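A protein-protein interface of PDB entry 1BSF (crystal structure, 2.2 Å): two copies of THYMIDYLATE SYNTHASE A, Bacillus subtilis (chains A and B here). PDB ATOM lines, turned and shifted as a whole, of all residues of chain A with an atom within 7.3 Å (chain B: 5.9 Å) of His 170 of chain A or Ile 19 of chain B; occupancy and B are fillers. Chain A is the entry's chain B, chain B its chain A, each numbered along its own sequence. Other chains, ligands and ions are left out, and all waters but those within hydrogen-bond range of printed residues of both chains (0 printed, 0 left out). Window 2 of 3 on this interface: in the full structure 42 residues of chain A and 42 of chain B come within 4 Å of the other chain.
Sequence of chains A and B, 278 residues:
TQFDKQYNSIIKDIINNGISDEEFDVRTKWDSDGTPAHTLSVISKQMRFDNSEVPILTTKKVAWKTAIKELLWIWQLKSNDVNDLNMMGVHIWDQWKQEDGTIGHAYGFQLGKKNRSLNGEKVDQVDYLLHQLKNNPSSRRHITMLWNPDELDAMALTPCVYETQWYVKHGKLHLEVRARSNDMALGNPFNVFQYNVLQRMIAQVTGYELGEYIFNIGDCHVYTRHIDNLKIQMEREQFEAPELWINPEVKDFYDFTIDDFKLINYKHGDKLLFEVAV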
ATOM      1  N   TYR A 167     -18.492  22.974 -21.048  1.00  0.00           N
ATOM      2  CA  TYR A 167     -18.725  22.505 -22.399  1.00  0.00           C
ATOM      3  C   TYR A 167     -17.720  21.386 -22.690  1.00  0.00           C
ATOM      4  O   TYR A 167     -16.569  21.445 -22.264  1.00  0.00           O
ATOM      5  CB  TYR A 167     -18.540  23.648 -23.409  1.00  0.00           C
ATOM      6  CG  TYR A 167     -19.276  24.944 -23.091  1.00  0.00           C
ATOM      7  CD1 TYR A 167     -20.586  25.152 -23.511  1.00  0.00           C
ATOM      8  CD2 TYR A 167     -18.649  25.972 -22.390  1.00  0.00           C
ATOM      9  CE1 TYR A 167     -21.252  26.355 -23.237  1.00  0.00           C
ATOM     10  CE2 TYR A 167     -19.307  27.174 -22.113  1.00  0.00           C
ATOM     11  CZ  TYR A 167     -20.600  27.361 -22.532  1.00  0.00           C
ATOM     12  OH  TYR A 167     -21.249  28.542 -22.222  1.00  0.00           O
ATOM     13  N   VAL A 168     -18.171  20.354 -23.389  1.00  0.00           N
ATOM     14  CA  VAL A 168     -17.314  19.237 -23.773  1.00  0.00           C
ATOM     15  C   VAL A 168     -17.241  19.250 -25.297  1.00  0.00           C
ATOM     16  O   VAL A 168     -18.092  18.676 -25.976  1.00  0.00           O
ATOM     17  CB  VAL A 168     -17.910  17.898 -23.365  1.00  0.00           C
ATOM     18  CG1 VAL A 168     -17.075  16.768 -23.929  1.00  0.00           C
ATOM     19  CG2 VAL A 168     -17.993  17.814 -21.872  1.00  0.00           C
ATOM     20  N   LYS A 169     -16.222  19.905 -25.835  1.00  0.00           N
ATOM     21  CA  LYS A 169     -16.064  19.982 -27.276  1.00  0.00           C
ATOM     22  C   LYS A 169     -14.695  19.487 -27.737  1.00  0.00           C
ATOM     23  O   LYS A 169     -13.662  20.075 -27.415  1.00  0.00           O
ATOM     24  CB  LYS A 169     -16.307  21.422 -27.722  1.00  0.00           C
ATOM     25  CG  LYS A 169     -17.669  21.954 -27.274  1.00  0.00           C
ATOM     26  CD  LYS A 169     -18.169  23.078 -28.167  1.00  0.00           C
ATOM     27  CE  LYS A 169     -19.581  23.515 -27.784  1.00  0.00           C
ATOM     28  NZ  LYS A 169     -20.331  23.933 -29.000  1.00  0.00           N
ATOM     29  N   HIS A 170     -14.704  18.387 -28.486  1.00  0.00           N
ATOM     30  CA  HIS A 170     -13.483  17.787 -29.016  1.00  0.00           C
ATOM     31  C   HIS A 170     -12.533  17.347 -27.910  1.00  0.00           C
ATOM     32  O   HIS A 170     -11.444  17.894 -27.767  1.00  0.00           O
ATOM     33  CB  HIS A 170     -12.765  18.777 -29.946  1.00  0.00           C
ATOM     34  CG  HIS A 170     -13.393  18.904 -31.300  1.00  0.00           C
ATOM     35  ND1 HIS A 170     -14.583  18.289 -31.631  1.00  0.00           N
ATOM     36  CD2 HIS A 170     -12.996  19.576 -32.408  1.00  0.00           C
ATOM     37  CE1 HIS A 170     -14.892  18.578 -32.883  1.00  0.00           C
ATOM     38  NE2 HIS A 170     -13.946  19.356 -33.377  1.00  0.00           N
ATOM     39  N   GLY A 171     -12.947  16.355 -27.132  1.00  0.00           N
ATOM     40  CA  GLY A 171     -12.110  15.866 -26.051  1.00  0.00           C
ATOM     41  C   GLY A 171     -11.629  16.974 -25.135  1.00  0.00           C
ATOM     42  O   GLY A 171     -10.724  16.772 -24.316  1.00  0.00           O
ATOM     43  N   LYS A 172     -12.230  18.152 -25.277  1.00  0.00           N
ATOM     44  CA  LYS A 172     -11.856  19.284 -24.448  1.00  0.00           C
ATOM     45  C   LYS A 172     -12.982  19.731 -23.541  1.00  0.00           C
ATOM     46  O   LYS A 172     -14.150  19.668 -23.904  1.00  0.00           O
ATOM     47  CB  LYS A 172     -11.410  20.455 -25.309  1.00  0.00           C
ATOM     48  CG  LYS A 172     -10.119  21.091 -24.826  1.00  0.00           C
ATOM     49  CD  LYS A 172      -9.105  21.205 -25.955  1.00  0.00           C
ATOM     50  CE  LYS A 172      -8.715  19.834 -26.480  1.00  0.00           C
ATOM     51  NZ  LYS A 172      -7.867  19.925 -27.696  1.00  0.00           N
ATOM     52  N   LEU A 173     -12.602  20.185 -22.354  1.00  0.00           N
ATOM     53  CA  LEU A 173     -13.536  20.658 -21.347  1.00  0.00           C
ATOM     54  C   LEU A 173     -13.325  22.156 -21.177  1.00  0.00           C
ATOM     55  O   LEU A 173     -12.237  22.602 -20.802  1.00  0.00           O
ATOM     56  CB  LEU A 173     -13.267  19.940 -20.024  1.00  0.00           C
ATOM     57  CG  LEU A 173     -14.078  20.216 -18.752  1.00  0.00           C
ATOM     58  CD1 LEU A 173     -15.059  21.348 -18.948  1.00  0.00           C
ATOM     59  CD2 LEU A 173     -14.806  18.946 -18.365  1.00  0.00           C
ATOM     60  N   HIS A 174     -14.363  22.933 -21.462  1.00  0.00           N
ATOM     61  CA  HIS A 174     -14.262  24.379 -21.317  1.00  0.00           C
ATOM     62  C   HIS A 174     -15.074  24.813 -20.108  1.00  0.00           C
ATOM     63  O   HIS A 174     -16.183  24.316 -19.864  1.00  0.00           O
ATOM     64  CB  HIS A 174     -14.766  25.088 -22.575  1.00  0.00           C
ATOM     65  CG  HIS A 174     -14.100  24.630 -23.835  1.00  0.00           C
ATOM     66  ND1 HIS A 174     -13.058  25.318 -24.415  1.00  0.00           N
ATOM     67  CD2 HIS A 174     -14.338  23.562 -24.633  1.00  0.00           C
ATOM     68  CE1 HIS A 174     -12.685  24.695 -25.519  1.00  0.00           C
ATOM     69  NE2 HIS A 174     -13.444  23.627 -25.672  1.00  0.00           N
ATOM     70  N   TYR A 208     -10.736  14.379 -19.830  1.00  0.00           N
ATOM     71  CA  TYR A 208     -10.933  15.266 -20.972  1.00  0.00           C
ATOM     72  C   TYR A 208      -9.866  16.340 -20.908  1.00  0.00           C
ATOM     73  O   TYR A 208      -9.575  16.851 -19.831  1.00  0.00           O
ATOM     74  CB  TYR A 208     -12.292  15.958 -20.901  1.00  0.00           C
ATOM     75  CG  TYR A 208     -13.460  15.132 -21.362  1.00  0.00           C
ATOM     76  CD1 TYR A 208     -13.727  14.961 -22.720  1.00  0.00           C
ATOM     77  CD2 TYR A 208     -14.337  14.577 -20.445  1.00  0.00           C
ATOM     78  CE1 TYR A 208     -14.850  14.254 -23.152  1.00  0.00           C
ATOM     79  CE2 TYR A 208     -15.457  13.873 -20.858  1.00  0.00           C
ATOM     80  CZ  TYR A 208     -15.714  13.714 -22.212  1.00  0.00           C
ATOM     81  OH  TYR A 208     -16.846  13.033 -22.616  1.00  0.00           O
ATOM     82  N   GLU A 209      -9.292  16.684 -22.053  1.00  0.00           N
ATOM     83  CA  GLU A 209      -8.270  17.720 -22.105  1.00  0.00           C
ATOM     84  C   GLU A 209      -8.916  19.033 -21.661  1.00  0.00           C
ATOM     85  O   GLU A 209     -10.142  19.179 -21.707  1.00  0.00           O
ATOM     86  CB  GLU A 209      -7.744  17.863 -23.532  1.00  0.00           C
ATOM     87  CG  GLU A 209      -6.488  17.061 -23.825  1.00  0.00           C
ATOM     88  CD  GLU A 209      -5.720  17.617 -25.015  1.00  0.00           C
ATOM     89  OE1 GLU A 209      -6.355  17.847 -26.061  1.00  0.00           O
ATOM     90  OE2 GLU A 209      -4.490  17.831 -24.909  1.00  0.00           O
ATOM     91  N   ILE B  14     -18.764  31.939 -36.456  1.00  0.00           N
ATOM     92  CA  ILE B  14     -19.270  30.603 -36.163  1.00  0.00           C
ATOM     93  C   ILE B  14     -19.079  29.658 -37.339  1.00  0.00           C
ATOM     94  O   ILE B  14     -18.749  28.487 -37.160  1.00  0.00           O
ATOM     95  CB  ILE B  14     -20.750  30.668 -35.792  1.00  0.00           C
ATOM     96  CG1 ILE B  14     -20.917  31.620 -34.609  1.00  0.00           C
ATOM     97  CG2 ILE B  14     -21.288  29.267 -35.505  1.00  0.00           C
ATOM     98  CD1 ILE B  14     -22.357  31.913 -34.233  1.00  0.00           C
ATOM     99  N   ASN B  17     -15.029  29.721 -37.275  1.00  0.00           N
ATOM    100  CA  ASN B  17     -14.371  29.220 -36.060  1.00  0.00           C
ATOM    101  C   ASN B  17     -15.204  28.226 -35.224  1.00  0.00           C
ATOM    102  O   ASN B  17     -14.707  27.667 -34.240  1.00  0.00           O
ATOM    103  CB  ASN B  17     -13.959  30.395 -35.159  1.00  0.00           C
ATOM    104  CG  ASN B  17     -12.845  31.243 -35.752  1.00  0.00           C
ATOM    105  OD1 ASN B  17     -11.702  30.794 -35.900  1.00  0.00           O
ATOM    106  ND2 ASN B  17     -13.172  32.485 -36.082  1.00  0.00           N
ATOM    107  N   GLY B  18     -16.458  28.010 -35.606  1.00  0.00           N
ATOM    108  CA  GLY B  18     -17.313  27.091 -34.869  1.00  0.00           C
ATOM    109  C   GLY B  18     -16.943  25.618 -34.970  1.00  0.00           C
ATOM    110  O   GLY B  18     -16.385  25.177 -35.975  1.00  0.00           O
ATOM    111  N   ILE B  19     -17.285  24.853 -33.937  1.00  0.00           N
ATOM    112  CA  ILE B  19     -16.979  23.425 -33.875  1.00  0.00           C
ATOM    113  C   ILE B  19     -18.229  22.578 -34.063  1.00  0.00           C
ATOM    114  O   ILE B  19     -19.224  22.766 -33.363  1.00  0.00           O
ATOM    115  CB  ILE B  19     -16.385  23.053 -32.507  1.00  0.00           C
ATOM    116  CG1 ILE B  19     -15.113  23.860 -32.243  1.00  0.00           C
ATOM    117  CG2 ILE B  19     -16.128  21.557 -32.446  1.00  0.00           C
ATOM    118  CD1 ILE B  19     -14.765  23.973 -30.763  1.00  0.00           C
ATOM    119  N   SER B  20     -18.168  21.609 -34.969  1.00  0.00           N
ATOM    120  CA  SER B  20     -19.332  20.769 -35.217  1.00  0.00           C
ATOM    121  C   SER B  20     -19.712  19.820 -34.094  1.00  0.00           C
ATOM    122  O   SER B  20     -18.866  19.147 -33.512  1.00  0.00           O
ATOM    123  CB  SER B  20     -19.154  19.969 -36.507  1.00  0.00           C
ATOM    124  OG  SER B  20     -20.244  20.201 -37.392  1.00  0.00           O
ATOM    125  N   ASP B  21     -21.012  19.772 -33.815  1.00  0.00           N
ATOM    126  CA  ASP B  21     -21.573  18.909 -32.781  1.00  0.00           C
ATOM    127  C   ASP B  21     -21.470  17.445 -33.212  1.00  0.00           C
ATOM    128  O   ASP B  21     -21.637  16.524 -32.403  1.00  0.00           O
ATOM    129  CB  ASP B  21     -23.048  19.274 -32.544  1.00  0.00           C
ATOM    130  CG  ASP B  21     -23.944  18.952 -33.747  1.00  0.00           C
ATOM    131  OD1 ASP B  21     -23.438  18.866 -34.882  1.00  0.00           O
ATOM    132  OD2 ASP B  21     -25.162  18.781 -33.557  1.00  0.00           O
ATOM    133  N   GLU B  23     -19.515  14.810 -33.684  1.00  0.00           N
ATOM    134  CA  GLU B  23     -19.010  13.770 -32.796  1.00  0.00           C
ATOM    135  C   GLU B  23     -20.062  13.137 -31.900  1.00  0.00           C
ATOM    136  O   GLU B  23     -19.814  12.085 -31.311  1.00  0.00           O
ATOM    137  CB  GLU B  23     -17.891  14.336 -31.922  1.00  0.00           C
ATOM    138  CG  GLU B  23     -17.516  15.770 -32.263  1.00  0.00           C
ATOM    139  CD  GLU B  23     -17.445  16.664 -31.042  1.00  0.00           C
ATOM    140  OE1 GLU B  23     -17.289  16.131 -29.925  1.00  0.00           O
ATOM    141  OE2 GLU B  23     -17.543  17.900 -31.203  1.00  0.00           O
ATOM    142  N   PHE B  24     -21.232  13.758 -31.793  1.00  0.00           N
ATOM    143  CA  PHE B  24     -22.273  13.226 -30.932  1.00  0.00           C
ATOM    144  C   PHE B  24     -23.531  12.748 -31.645  1.00  0.00           C
ATOM    145  O   PHE B  24     -23.728  13.011 -32.836  1.00  0.00           O
ATOM    146  CB  PHE B  24     -22.635  14.272 -29.881  1.00  0.00           C
ATOM    147  CG  PHE B  24     -21.487  14.643 -28.981  1.00  0.00           C
ATOM    148  CD1 PHE B  24     -20.988  13.728 -28.049  1.00  0.00           C
ATOM    149  CD2 PHE B  24     -20.893  15.902 -29.068  1.00  0.00           C
ATOM    150  CE1 PHE B  24     -19.920  14.061 -27.223  1.00  0.00           C
ATOM    151  CE2 PHE B  24     -19.822  16.241 -28.239  1.00  0.00           C
ATOM    152  CZ  PHE B  24     -19.337  15.319 -27.317  1.00  0.00           C
ATOM    153  N   THR B  39     -25.053  21.071 -36.260  1.00  0.00           N
ATOM    154  CA  THR B  39     -24.615  22.450 -36.078  1.00  0.00           C
ATOM    155  C   THR B  39     -23.103  22.692 -35.887  1.00  0.00           C
ATOM    156  O   THR B  39     -22.296  21.758 -35.833  1.00  0.00           O
ATOM    157  CB  THR B  39     -25.349  23.059 -34.854  1.00  0.00           C
ATOM    158  OG1 THR B  39     -24.535  22.908 -33.680  1.00  0.00           O
ATOM    159  CG2 THR B  39     -26.661  22.334 -34.602  1.00  0.00           C
ATOM    160  N   LEU B  40     -22.745  23.973 -35.806  1.00  0.00           N
ATOM    161  CA  LEU B  40     -21.376  24.414 -35.559  1.00  0.00           C
ATOM    162  C   LEU B  40     -21.549  25.402 -34.409  1.00  0.00           C
ATOM    163  O   LEU B  40     -22.580  26.068 -34.316  1.00  0.00           O
ATOM    164  CB  LEU B  40     -20.798  25.125 -36.777  1.00  0.00           C
ATOM    165  CG  LEU B  40     -20.512  24.217 -37.977  1.00  0.00           C
ATOM    166  CD1 LEU B  40     -21.095  24.856 -39.207  1.00  0.00           C
ATOM    167  CD2 LEU B  40     -19.008  24.001 -38.151  1.00  0.00           C
ATOM    168  N   SER B  41     -20.558  25.514 -33.535  1.00  0.00           N
ATOM    169  CA  SER B  41     -20.713  26.420 -32.405  1.00  0.00           C
ATOM    170  C   SER B  41     -19.440  27.015 -31.823  1.00  0.00           C
ATOM    171  O   SER B  41     -18.329  26.560 -32.102  1.00  0.00           O
ATOM    172  CB  SER B  41     -21.479  25.705 -31.287  1.00  0.00           C
ATOM    173  OG  SER B  41     -21.241  24.302 -31.319  1.00  0.00           O
ATOM    174  N   VAL B  42     -19.635  28.051 -31.009  1.00  0.00           N
ATOM    175  CA  VAL B  42     -18.549  28.734 -30.313  1.00  0.00           C
ATOM    176  C   VAL B  42     -19.011  29.001 -28.884  1.00  0.00           C
ATOM    177  O   VAL B  42     -20.195  29.165 -28.617  1.00  0.00           O
ATOM    178  CB  VAL B  42     -18.179  30.094 -30.959  1.00  0.00           C
ATOM    179  CG1 VAL B  42     -17.932  29.929 -32.459  1.00  0.00           C
ATOM    180  CG2 VAL B  42     -19.256  31.120 -30.668  1.00  0.00           C
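The side-chain amino group of Lys 169 of chain A sits at hydrogen-bond distance from the side-chain hydroxyl of Ser 41 of chain B. The side-chain carboxylate (OE2) of Glu 23 of chain B is in hydrogen-bond range of a ring nitrogen (ND1) of His 170 of chain A, at 3.0 Å.
The backbone carbonyl oxygen (O) of Ser 41 of chain B is in hydrogen-bond range of the backbone NH (N) of Ile 19 of chain B.
Val 168 of chain A touches Phe 24 of chain B (O to CE2, 3.7 Å). Ile 19 of chain B touches His 170 of chain A (CG2 to NE2, 3.2 Å).
His 170 of chain A touches just these residues of chain B: Ile 19 (3.2 Å) and Glu 23 (3.0 Å). Ile 19 of chain B touches one residue of chain A. Of the printed residues of chain A, Glu 23 of chain B touches His 170. Printed residues of chain A within 4 Å of Phe 24 of chain B: Val 168 (3.7 Å). The nearest residue of chain B that does not touch His 170 of chain A is Ser 20 of chain B (4.1 Å). The nearest residue of chain A that does not touch Ile 19 of chain B is Lys 169 of chain A (4.3 Å). The nearest printed residue of chain B that does not touch Lys 169 of chain A is Ile 19 of chain B (4.3 Å).
Hydrophobic or aromatic side chains of chain A that line the printed part of chain B: His 170. Of the 12 printed residues of chain B, 4 touch a printed residue of chain A. Hydrophobic or aromatic side chains of chain B within 4 Å of the printed part of chain A: Ile 19 and Phe 24. Among the printed residues, no Asp or Glu carboxylate lies within 4 Å of a Lys or Arg side-chain nitrogen of the other chain.
No position is printed for both chains. Of the 4 pairs that touch across the chains among the printed residues, none has its exchanged pair printed and touching as well.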
